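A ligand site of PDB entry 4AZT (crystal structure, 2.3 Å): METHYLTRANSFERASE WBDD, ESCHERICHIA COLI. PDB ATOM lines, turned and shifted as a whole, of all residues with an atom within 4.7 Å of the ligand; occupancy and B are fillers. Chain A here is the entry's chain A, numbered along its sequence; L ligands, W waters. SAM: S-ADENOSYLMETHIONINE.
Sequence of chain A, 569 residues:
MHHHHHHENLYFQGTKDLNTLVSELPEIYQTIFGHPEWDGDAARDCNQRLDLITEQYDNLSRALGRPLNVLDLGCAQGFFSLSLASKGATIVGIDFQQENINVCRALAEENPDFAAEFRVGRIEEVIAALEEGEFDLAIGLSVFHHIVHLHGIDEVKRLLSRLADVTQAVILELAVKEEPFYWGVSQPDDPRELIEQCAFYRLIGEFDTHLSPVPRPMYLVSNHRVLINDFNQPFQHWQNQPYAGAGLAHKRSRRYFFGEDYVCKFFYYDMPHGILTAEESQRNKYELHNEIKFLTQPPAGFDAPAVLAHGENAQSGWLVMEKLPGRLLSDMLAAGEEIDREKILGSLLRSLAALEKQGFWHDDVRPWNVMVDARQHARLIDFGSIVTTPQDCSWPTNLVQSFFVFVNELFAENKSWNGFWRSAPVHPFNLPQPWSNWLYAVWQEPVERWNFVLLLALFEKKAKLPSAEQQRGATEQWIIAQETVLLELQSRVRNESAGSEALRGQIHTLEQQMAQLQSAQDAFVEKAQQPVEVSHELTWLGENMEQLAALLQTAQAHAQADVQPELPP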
ATOM      1  N   TYR A  29      31.694 -24.211  11.515  1.00  0.00           N
ATOM      2  CA  TYR A  29      30.652 -23.288  11.840  1.00  0.00           C
ATOM      3  C   TYR A  29      29.987 -23.686  13.204  1.00  0.00           C
ATOM      4  O   TYR A  29      29.766 -22.843  14.079  1.00  0.00           O
ATOM      5  CB  TYR A  29      29.642 -23.224  10.670  1.00  0.00           C
ATOM      6  CG  TYR A  29      28.663 -22.089  10.796  1.00  0.00           C
ATOM      7  CD1 TYR A  29      28.968 -20.782  10.323  1.00  0.00           C
ATOM      8  CD2 TYR A  29      27.468 -22.280  11.457  1.00  0.00           C
ATOM      9  CE1 TYR A  29      28.071 -19.690  10.492  1.00  0.00           C
ATOM     10  CE2 TYR A  29      26.568 -21.228  11.632  1.00  0.00           C
ATOM     11  CZ  TYR A  29      26.871 -19.955  11.174  1.00  0.00           C
ATOM     12  OH  TYR A  29      25.907 -18.985  11.354  1.00  0.00           O
ATOM     13  N   GLN A  30      29.686 -24.973  13.379  1.00  0.00           N
ATOM     14  CA  GLN A  30      28.940 -25.401  14.541  1.00  0.00           C
ATOM     15  C   GLN A  30      29.848 -26.329  15.382  1.00  0.00           C
ATOM     16  O   GLN A  30      30.816 -26.862  14.877  1.00  0.00           O
ATOM     17  CB  GLN A  30      27.739 -26.275  14.121  1.00  0.00           C
ATOM     18  CG  GLN A  30      26.750 -25.689  13.110  1.00  0.00           C
ATOM     19  CD  GLN A  30      25.766 -26.733  12.699  1.00  0.00           C
ATOM     20  OE1 GLN A  30      26.147 -27.922  12.557  1.00  0.00           O
ATOM     21  NE2 GLN A  30      24.486 -26.347  12.542  1.00  0.00           N
ATOM     22  N   ARG A  44      30.097 -21.017  16.280  1.00  0.00           N
ATOM     23  CA  ARG A  44      28.898 -20.811  17.097  1.00  0.00           C
ATOM     24  C   ARG A  44      28.698 -22.048  17.945  1.00  0.00           C
ATOM     25  O   ARG A  44      28.616 -23.170  17.412  1.00  0.00           O
ATOM     26  CB  ARG A  44      27.669 -20.598  16.178  1.00  0.00           C
ATOM     27  CG  ARG A  44      27.895 -19.387  15.234  1.00  0.00           C
ATOM     28  CD  ARG A  44      26.645 -18.886  14.535  1.00  0.00           C
ATOM     29  NE  ARG A  44      25.626 -18.422  15.495  1.00  0.00           N
ATOM     30  CZ  ARG A  44      24.395 -18.059  15.136  1.00  0.00           C
ATOM     31  NH1 ARG A  44      24.010 -18.124  13.835  1.00  0.00           N
ATOM     32  NH2 ARG A  44      23.552 -17.665  16.080  1.00  0.00           N
ATOM     33  N   CYS A  46      26.005 -23.023  19.487  1.00  0.00           N
ATOM     34  CA  CYS A  46      24.720 -23.634  19.168  1.00  0.00           C
ATOM     35  C   CYS A  46      23.830 -24.016  20.352  1.00  0.00           C
ATOM     36  O   CYS A  46      22.675 -24.401  20.102  1.00  0.00           O
ATOM     37  CB  CYS A  46      24.887 -24.855  18.266  1.00  0.00           C
ATOM     38  SG  CYS A  46      25.656 -24.536  16.639  1.00  0.00           S
ATOM     39  N   ARG A  49      20.535 -21.582  20.679  1.00  0.00           N
ATOM     40  CA  ARG A  49      19.552 -21.938  19.640  1.00  0.00           C
ATOM     41  C   ARG A  49      18.985 -23.318  19.902  1.00  0.00           C
ATOM     42  O   ARG A  49      17.775 -23.463  19.910  1.00  0.00           O
ATOM     43  CB  ARG A  49      20.118 -21.763  18.227  1.00  0.00           C
ATOM     44  CG  ARG A  49      20.452 -20.255  17.964  1.00  0.00           C
ATOM     45  CD  ARG A  49      21.097 -20.017  16.599  1.00  0.00           C
ATOM     46  NE  ARG A  49      22.331 -20.790  16.440  1.00  0.00           N
ATOM     47  CZ  ARG A  49      22.780 -21.201  15.260  1.00  0.00           C
ATOM     48  NH1 ARG A  49      22.066 -20.929  14.153  1.00  0.00           N
ATOM     49  NH2 ARG A  49      23.906 -21.935  15.177  1.00  0.00           N
ATOM     50  N   LEU A  73      17.698 -27.240   6.665  1.00  0.00           N
ATOM     51  CA  LEU A  73      18.173 -26.611   5.432  1.00  0.00           C
ATOM     52  C   LEU A  73      19.459 -25.843   5.650  1.00  0.00           C
ATOM     53  O   LEU A  73      19.485 -24.871   6.422  1.00  0.00           O
ATOM     54  CB  LEU A  73      17.108 -25.617   4.930  1.00  0.00           C
ATOM     55  CG  LEU A  73      15.852 -26.384   4.440  1.00  0.00           C
ATOM     56  CD1 LEU A  73      14.684 -25.444   4.218  1.00  0.00           C
ATOM     57  CD2 LEU A  73      16.129 -27.215   3.220  1.00  0.00           C
ATOM     58  N   GLY A  74      20.500 -26.223   4.929  1.00  0.00           N
ATOM     59  CA  GLY A  74      21.806 -25.632   5.173  1.00  0.00           C
ATOM     60  C   GLY A  74      22.335 -26.112   6.534  1.00  0.00           C
ATOM     61  O   GLY A  74      22.738 -25.286   7.352  1.00  0.00           O
ATOM     62  N   CYS A  75      22.368 -27.436   6.721  1.00  0.00           N
ATOM     63  CA  CYS A  75      22.533 -28.060   8.034  1.00  0.00           C
ATOM     64  C   CYS A  75      23.976 -28.058   8.527  1.00  0.00           C
ATOM     65  O   CYS A  75      24.266 -28.451   9.699  1.00  0.00           O
ATOM     66  CB  CYS A  75      22.044 -29.520   7.946  1.00  0.00           C
ATOM     67  SG  CYS A  75      22.978 -30.567   6.778  1.00  0.00           S
ATOM     68  N   ALA A  76      24.902 -27.668   7.642  1.00  0.00           N
ATOM     69  CA  ALA A  76      26.337 -27.422   8.029  1.00  0.00           C
ATOM     70  C   ALA A  76      26.930 -28.728   8.586  1.00  0.00           C
ATOM     71  O   ALA A  76      26.943 -29.747   7.862  1.00  0.00           O
ATOM     72  CB  ALA A  76      26.458 -26.267   9.008  1.00  0.00           C
ATOM     73  N   PHE A  80      22.172 -29.535  14.828  1.00  0.00           N
ATOM     74  CA  PHE A  80      20.767 -29.522  15.220  1.00  0.00           C
ATOM     75  C   PHE A  80      20.053 -30.763  14.749  1.00  0.00           C
ATOM     76  O   PHE A  80      19.126 -31.235  15.404  1.00  0.00           O
ATOM     77  CB  PHE A  80      20.035 -28.265  14.658  1.00  0.00           C
ATOM     78  CG  PHE A  80      20.602 -26.991  15.173  1.00  0.00           C
ATOM     79  CD1 PHE A  80      20.191 -26.487  16.393  1.00  0.00           C
ATOM     80  CD2 PHE A  80      21.598 -26.328  14.478  1.00  0.00           C
ATOM     81  CE1 PHE A  80      20.762 -25.321  16.918  1.00  0.00           C
ATOM     82  CE2 PHE A  80      22.156 -25.148  14.967  1.00  0.00           C
ATOM     83  CZ  PHE A  80      21.756 -24.654  16.206  1.00  0.00           C
ATOM     84  N   ILE A  94      20.273 -31.042   4.752  1.00  0.00           N
ATOM     85  CA  ILE A  94      20.658 -30.648   3.429  1.00  0.00           C
ATOM     86  C   ILE A  94      21.697 -29.557   3.516  1.00  0.00           C
ATOM     87  O   ILE A  94      21.509 -28.573   4.250  1.00  0.00           O
ATOM     88  CB  ILE A  94      19.439 -30.040   2.719  1.00  0.00           C
ATOM     89  CG1 ILE A  94      18.327 -31.097   2.646  1.00  0.00           C
ATOM     90  CG2 ILE A  94      19.798 -29.566   1.307  1.00  0.00           C
ATOM     91  CD1 ILE A  94      18.586 -32.131   1.590  1.00  0.00           C
ATOM     92  N   ASP A  95      22.783 -29.696   2.766  1.00  0.00           N
ATOM     93  CA  ASP A  95      23.768 -28.621   2.639  1.00  0.00           C
ATOM     94  C   ASP A  95      24.440 -28.671   1.273  1.00  0.00           C
ATOM     95  O   ASP A  95      24.607 -29.798   0.732  1.00  0.00           O
ATOM     96  CB  ASP A  95      24.864 -28.780   3.738  1.00  0.00           C
ATOM     97  CG  ASP A  95      25.558 -27.475   4.030  1.00  0.00           C
ATOM     98  OD1 ASP A  95      26.550 -27.198   3.298  1.00  0.00           O
ATOM     99  OD2 ASP A  95      25.066 -26.700   4.921  1.00  0.00           O
ATOM    100  N   PHE A  96      24.812 -27.536   0.691  1.00  0.00           N
ATOM    101  CA  PHE A  96      25.454 -27.668  -0.633  1.00  0.00           C
ATOM    102  C   PHE A  96      26.985 -27.853  -0.662  1.00  0.00           C
ATOM    103  O   PHE A  96      27.550 -27.828  -1.736  1.00  0.00           O
ATOM    104  CB  PHE A  96      25.023 -26.615  -1.687  1.00  0.00           C
ATOM    105  CG  PHE A  96      25.531 -25.215  -1.436  1.00  0.00           C
ATOM    106  CD1 PHE A  96      26.204 -24.883  -0.260  1.00  0.00           C
ATOM    107  CD2 PHE A  96      25.268 -24.186  -2.365  1.00  0.00           C
ATOM    108  CE1 PHE A  96      26.648 -23.577  -0.021  1.00  0.00           C
ATOM    109  CE2 PHE A  96      25.704 -22.881  -2.137  1.00  0.00           C
ATOM    110  CZ  PHE A  96      26.414 -22.575  -0.967  1.00  0.00           C
ATOM    111  N   GLN A  97      27.641 -27.977   0.495  1.00  0.00           N
ATOM    112  CA  GLN A  97      29.070 -28.249   0.553  1.00  0.00           C
ATOM    113  C   GLN A  97      29.303 -29.705   0.927  1.00  0.00           C
ATOM    114  O   GLN A  97      28.908 -30.171   2.000  1.00  0.00           O
ATOM    115  CB  GLN A  97      29.773 -27.330   1.552  1.00  0.00           C
ATOM    116  CG  GLN A  97      29.886 -25.897   1.065  1.00  0.00           C
ATOM    117  CD  GLN A  97      30.585 -25.009   2.063  1.00  0.00           C
ATOM    118  OE1 GLN A  97      31.820 -25.077   2.159  1.00  0.00           O
ATOM    119  NE2 GLN A  97      29.833 -24.168   2.811  1.00  0.00           N
ATOM    120  N   ASN A 100      30.713 -30.523   4.387  1.00  0.00           N
ATOM    121  CA  ASN A 100      29.828 -30.450   5.501  1.00  0.00           C
ATOM    122  C   ASN A 100      29.065 -31.755   5.571  1.00  0.00           C
ATOM    123  O   ASN A 100      28.954 -32.350   6.644  1.00  0.00           O
ATOM    124  CB  ASN A 100      28.866 -29.277   5.326  1.00  0.00           C
ATOM    125  CG  ASN A 100      29.535 -27.925   5.569  1.00  0.00           C
ATOM    126  OD1 ASN A 100      30.606 -27.856   6.179  1.00  0.00           O
ATOM    127  ND2 ASN A 100      28.851 -26.836   5.152  1.00  0.00           N
ATOM    128  N   GLY A 121      22.794 -30.864  -1.531  1.00  0.00           N
ATOM    129  CA  GLY A 121      21.790 -30.327  -2.464  1.00  0.00           C
ATOM    130  C   GLY A 121      21.613 -28.862  -2.207  1.00  0.00           C
ATOM    131  O   GLY A 121      22.104 -28.336  -1.202  1.00  0.00           O
ATOM    132  N   ARG A 122      20.975 -28.196  -3.146  1.00  0.00           N
ATOM    133  CA  ARG A 122      20.656 -26.784  -2.979  1.00  0.00           C
ATOM    134  C   ARG A 122      19.263 -26.659  -2.344  1.00  0.00           C
ATOM    135  O   ARG A 122      18.333 -27.376  -2.711  1.00  0.00           O
ATOM    136  CB  ARG A 122      20.712 -26.034  -4.315  1.00  0.00           C
ATOM    137  CG  ARG A 122      22.062 -25.448  -4.697  1.00  0.00           C
ATOM    138  CD  ARG A 122      21.925 -24.325  -5.757  1.00  0.00           C
ATOM    139  NE  ARG A 122      21.706 -22.954  -5.217  1.00  0.00           N
ATOM    140  CZ  ARG A 122      22.681 -22.080  -4.939  1.00  0.00           C
ATOM    141  NH1 ARG A 122      23.944 -22.434  -5.128  1.00  0.00           N
ATOM    142  NH2 ARG A 122      22.400 -20.869  -4.447  1.00  0.00           N
ATOM    143  N   ILE A 123      19.154 -25.755  -1.384  1.00  0.00           N
ATOM    144  CA  ILE A 123      17.898 -25.446  -0.723  1.00  0.00           C
ATOM    145  C   ILE A 123      16.759 -25.071  -1.712  1.00  0.00           C
ATOM    146  O   ILE A 123      15.616 -25.546  -1.595  1.00  0.00           O
ATOM    147  CB  ILE A 123      18.187 -24.308   0.274  1.00  0.00           C
ATOM    148  CG1 ILE A 123      19.046 -24.854   1.414  1.00  0.00           C
ATOM    149  CG2 ILE A 123      16.925 -23.676   0.792  1.00  0.00           C
ATOM    150  CD1 ILE A 123      19.543 -23.715   2.247  1.00  0.00           C
ATOM    151  N   GLU A 124      17.061 -24.261  -2.697  1.00  0.00           N
ATOM    152  CA  GLU A 124      16.070 -23.926  -3.738  1.00  0.00           C
ATOM    153  C   GLU A 124      15.464 -25.155  -4.416  1.00  0.00           C
ATOM    154  O   GLU A 124      14.245 -25.238  -4.558  1.00  0.00           O
ATOM    155  CB  GLU A 124      16.687 -22.965  -4.782  1.00  0.00           C
ATOM    156  CG  GLU A 124      17.353 -21.744  -4.140  1.00  0.00           C
ATOM    157  CD  GLU A 124      18.874 -21.918  -3.959  1.00  0.00           C
ATOM    158  OE1 GLU A 124      19.354 -22.934  -3.399  1.00  0.00           O
ATOM    159  OE2 GLU A 124      19.612 -21.023  -4.367  1.00  0.00           O
ATOM    160  N   LEU A 141      18.284 -21.929   9.574  1.00  0.00           N
ATOM    161  CA  LEU A 141      18.991 -20.994  10.444  1.00  0.00           C
ATOM    162  C   LEU A 141      20.142 -20.395   9.676  1.00  0.00           C
ATOM    163  O   LEU A 141      21.027 -21.147   9.261  1.00  0.00           O
ATOM    164  CB  LEU A 141      19.584 -21.749  11.649  1.00  0.00           C
ATOM    165  CG  LEU A 141      18.616 -22.691  12.297  1.00  0.00           C
ATOM    166  CD1 LEU A 141      19.228 -23.493  13.450  1.00  0.00           C
ATOM    167  CD2 LEU A 141      17.305 -21.955  12.670  1.00  0.00           C
ATOM    168  N   SER A 142      20.162 -19.059   9.527  1.00  0.00           N
ATOM    169  CA  SER A 142      21.284 -18.332   8.915  1.00  0.00           C
ATOM    170  C   SER A 142      21.688 -18.897   7.540  1.00  0.00           C
ATOM    171  O   SER A 142      22.892 -19.025   7.224  1.00  0.00           O
ATOM    172  CB  SER A 142      22.510 -18.378   9.815  1.00  0.00           C
ATOM    173  OG  SER A 142      22.314 -17.628  10.993  1.00  0.00           O
ATOM    174  N   VAL A 143      20.705 -19.253   6.731  1.00  0.00           N
ATOM    175  CA  VAL A 143      21.013 -19.760   5.430  1.00  0.00           C
ATOM    176  C   VAL A 143      20.343 -18.903   4.314  1.00  0.00           C
ATOM    177  O   VAL A 143      20.927 -18.709   3.231  1.00  0.00           O
ATOM    178  CB  VAL A 143      20.625 -21.245   5.331  1.00  0.00           C
ATOM    179  CG1 VAL A 143      19.106 -21.458   5.615  1.00  0.00           C
ATOM    180  CG2 VAL A 143      21.010 -21.760   3.955  1.00  0.00           C
ATOM    181  N   HIS A 146      21.922 -15.966   2.201  1.00  0.00           N
ATOM    182  CA  HIS A 146      22.733 -16.322   1.036  1.00  0.00           C
ATOM    183  C   HIS A 146      21.931 -16.392  -0.228  1.00  0.00           C
ATOM    184  O   HIS A 146      22.420 -15.992  -1.291  1.00  0.00           O
ATOM    185  CB  HIS A 146      23.465 -17.631   1.267  1.00  0.00           C
ATOM    186  CG  HIS A 146      24.522 -17.533   2.355  1.00  0.00           C
ATOM    187  ND1 HIS A 146      24.356 -18.101   3.589  1.00  0.00           N
ATOM    188  CD2 HIS A 146      25.767 -16.889   2.381  1.00  0.00           C
ATOM    189  CE1 HIS A 146      25.442 -17.843   4.342  1.00  0.00           C
ATOM    190  NE2 HIS A 146      26.298 -17.109   3.609  1.00  0.00           N
ATOM    191  N   ILE A 147      20.699 -16.924  -0.126  1.00  0.00           N
ATOM    192  CA  ILE A 147      19.801 -17.108  -1.269  1.00  0.00           C
ATOM    193  C   ILE A 147      19.234 -15.736  -1.622  1.00  0.00           C
ATOM    194  O   ILE A 147      18.954 -15.447  -2.790  1.00  0.00           O
ATOM    195  CB  ILE A 147      18.685 -18.145  -0.959  1.00  0.00           C
ATOM    196  CG1 ILE A 147      19.285 -19.514  -0.622  1.00  0.00           C
ATOM    197  CG2 ILE A 147      17.707 -18.320  -2.105  1.00  0.00           C
ATOM    198  CD1 ILE A 147      18.330 -20.451   0.086  1.00  0.00           C
ATOM    199  N   GLU A 173      16.166 -18.611  11.686  1.00  0.00           N
ATOM    200  CA  GLU A 173      17.033 -17.523  12.169  1.00  0.00           C
ATOM    201  C   GLU A 173      17.464 -16.693  10.969  1.00  0.00           C
ATOM    202  O   GLU A 173      18.071 -17.208  10.057  1.00  0.00           O
ATOM    203  CB  GLU A 173      18.292 -18.070  12.841  1.00  0.00           C
ATOM    204  CG  GLU A 173      19.209 -16.928  13.368  1.00  0.00           C
ATOM    205  CD  GLU A 173      20.502 -17.451  13.994  1.00  0.00           C
ATOM    206  OE1 GLU A 173      21.125 -18.363  13.360  1.00  0.00           O
ATOM    207  OE2 GLU A 173      20.866 -16.963  15.098  1.00  0.00           O
HETATM  208  N   SAM L   1      22.194 -23.649   9.504  1.00  0.00           N
HETATM  209  CA  SAM L   1      23.513 -23.845  10.122  1.00  0.00           C
HETATM  210  C   SAM L   1      23.493 -23.138  11.468  1.00  0.00           C
HETATM  211  O   SAM L   1      22.940 -22.030  11.607  1.00  0.00           O
HETATM  212  OXT SAM L   1      24.030 -23.673  12.447  1.00  0.00           O
HETATM  213  CB  SAM L   1      24.631 -23.278   9.241  1.00  0.00           C
HETATM  214  CG  SAM L   1      24.549 -21.793   8.901  1.00  0.00           C
HETATM  215  SD  SAM L   1      25.757 -21.261   7.850  1.00  0.00           S
HETATM  216  CE  SAM L   1      25.899 -19.613   7.996  1.00  0.00           C
HETATM  217  C5' SAM L   1      25.030 -21.426   6.312  1.00  0.00           C
HETATM  218  C4' SAM L   1      25.068 -22.895   5.795  1.00  0.00           C
HETATM  219  O4' SAM L   1      24.246 -23.060   4.647  1.00  0.00           O
HETATM  220  C3' SAM L   1      26.459 -23.281   5.292  1.00  0.00           C
HETATM  221  O3' SAM L   1      26.691 -24.578   5.833  1.00  0.00           O
HETATM  222  C2' SAM L   1      26.393 -23.396   3.758  1.00  0.00           C
HETATM  223  O2' SAM L   1      27.095 -24.543   3.246  1.00  0.00           O
HETATM  224  C1' SAM L   1      24.935 -23.750   3.563  1.00  0.00           C
HETATM  225  N9  SAM L   1      24.298 -23.202   2.371  1.00  0.00           N
HETATM  226  C8  SAM L   1      24.320 -21.883   1.993  1.00  0.00           C
HETATM  227  N7  SAM L   1      23.529 -21.681   0.908  1.00  0.00           N
HETATM  228  C5  SAM L   1      23.003 -22.889   0.594  1.00  0.00           C
HETATM  229  C6  SAM L   1      22.086 -23.388  -0.423  1.00  0.00           C
HETATM  230  N6  SAM L   1      21.630 -22.518  -1.356  1.00  0.00           N
HETATM  231  N1  SAM L   1      21.729 -24.679  -0.410  1.00  0.00           N
HETATM  232  C2  SAM L   1      22.225 -25.534   0.508  1.00  0.00           C
HETATM  233  N3  SAM L   1      23.068 -25.156   1.472  1.00  0.00           N
HETATM  234  C4  SAM L   1      23.503 -23.893   1.554  1.00  0.00           C
HETATM  235  O   HOH W   1      19.149 -24.549   9.028  1.00  0.00           O
HETATM  236  O   HOH W   2      28.398 -20.447   5.195  1.00  0.00           O
HETATM  237  O   HOH W   3      21.001 -25.864  11.121  1.00  0.00           O
HETATM  238  O   HOH W   4      29.200 -24.626   7.327  1.00  0.00           O
HETATM  239  O   HOH W   5      23.880 -19.291  -1.424  1.00  0.00           O
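O2' of the ligand is in hydrogen-bond range of OD1 of Asp 95 (2.7 Å).
NE2 of Gln 30 lies within hydrogen-bond range of OXT of the ligand (2.7 Å).
A nitrogen (N) of the ligand lies within hydrogen-bond range of the backbone carbonyl oxygen of Gly 74, at 2.8 Å.
A nitrogen (N) of the ligand sits at hydrogen-bond distance from the backbone carbonyl oxygen (O) of Leu 141 (2.8 Å).
O2' of the ligand sits at hydrogen-bond distance from NE2 of Gln 97 (2.8 Å).
O of the ligand lies within salt-bridge range of NH1 of Arg 49 (2.9 Å).
A nitrogen (N1) of the ligand is in hydrogen-bond range of the backbone NH (N) of Ile 123, at 3.0 Å.
N3 of the ligand lies within hydrogen-bond range of N of Phe 96, 3.1 Å away.
OE1 of Glu 124 is in hydrogen-bond range of N6 of the ligand.
O3' of the ligand lies within hydrogen-bond range of ND2 of Asn 100 (3.2 Å).
The side-chain carboxylate of Asp 95 is in hydrogen-bond range of the side-chain amide nitrogen of Asn 100 (3.0 Å).
The side-chain carboxylate of Asp 95 is in hydrogen-bond range of the backbone NH of Ala 76 (2.9 Å).
N of Cys 75 is in hydrogen-bond range of OD2 of Asp 95 (3.3 Å).
The guanidinium group of Arg 49 lies within salt-bridge range of the side-chain carboxylate of Glu 173.
The backbone carbonyl oxygen (O) of Gly 121 sits at hydrogen-bond distance from the backbone NH (N) of Phe 96, at 3.4 Å.
NH2 of Arg 122 is in salt-bridge range of OE2 of Glu 124 (2.8 Å).
OG of Ser 142 lies within hydrogen-bond range of OE1 of Glu 173 (2.7 Å).
O of Tyr 29 sits at hydrogen-bond distance from N of Arg 44 (2.9 Å).
A sulfur (SD) of the ligand lies close to the backbone carbonyl oxygen (O) of Ser 142, 3.7 Å away.
CE1 of Tyr 29 touches CE of the ligand, at 3.3 Å.
Ala 76 touches the ligand (CB to CB, 3.5 Å).
Phe 80 touches the ligand.
Gly 121 touches the ligand.
Arg 122 touches the ligand (CA to N1, 3.5 Å).
Val 143 touches the ligand.
Ile 147 touches the ligand (CG1 to N6, 3.9 Å).
Hydrophobic or aromatic side chains within 4 Å of the ligand: Tyr 29, Ala 76, Phe 80, Phe 96, Ile 123, Leu 141, Val 143 and Ile 147.
18 residues have an atom within 4 Å of the ligand: Tyr 29, Gln 30, Arg 49, Gly 74, Ala 76, Phe 80, Asp 95, Phe 96, Gln 97, Asn 100, Gly 121, Arg 122, Ile 123, Glu 124, Leu 141, Ser 142, Val 143 and Ile 147.
Water W4 lies within hydrogen-bond range of an oxygen (O3') of the ligand (2.9 Å) and the side-chain amide nitrogen of Asn 100 (3.1 Å).
Water W1 lies within hydrogen-bond range of the backbone carbonyl oxygen of Leu 73, the backbone NH of Leu 141 and a nitrogen (N) of the ligand.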
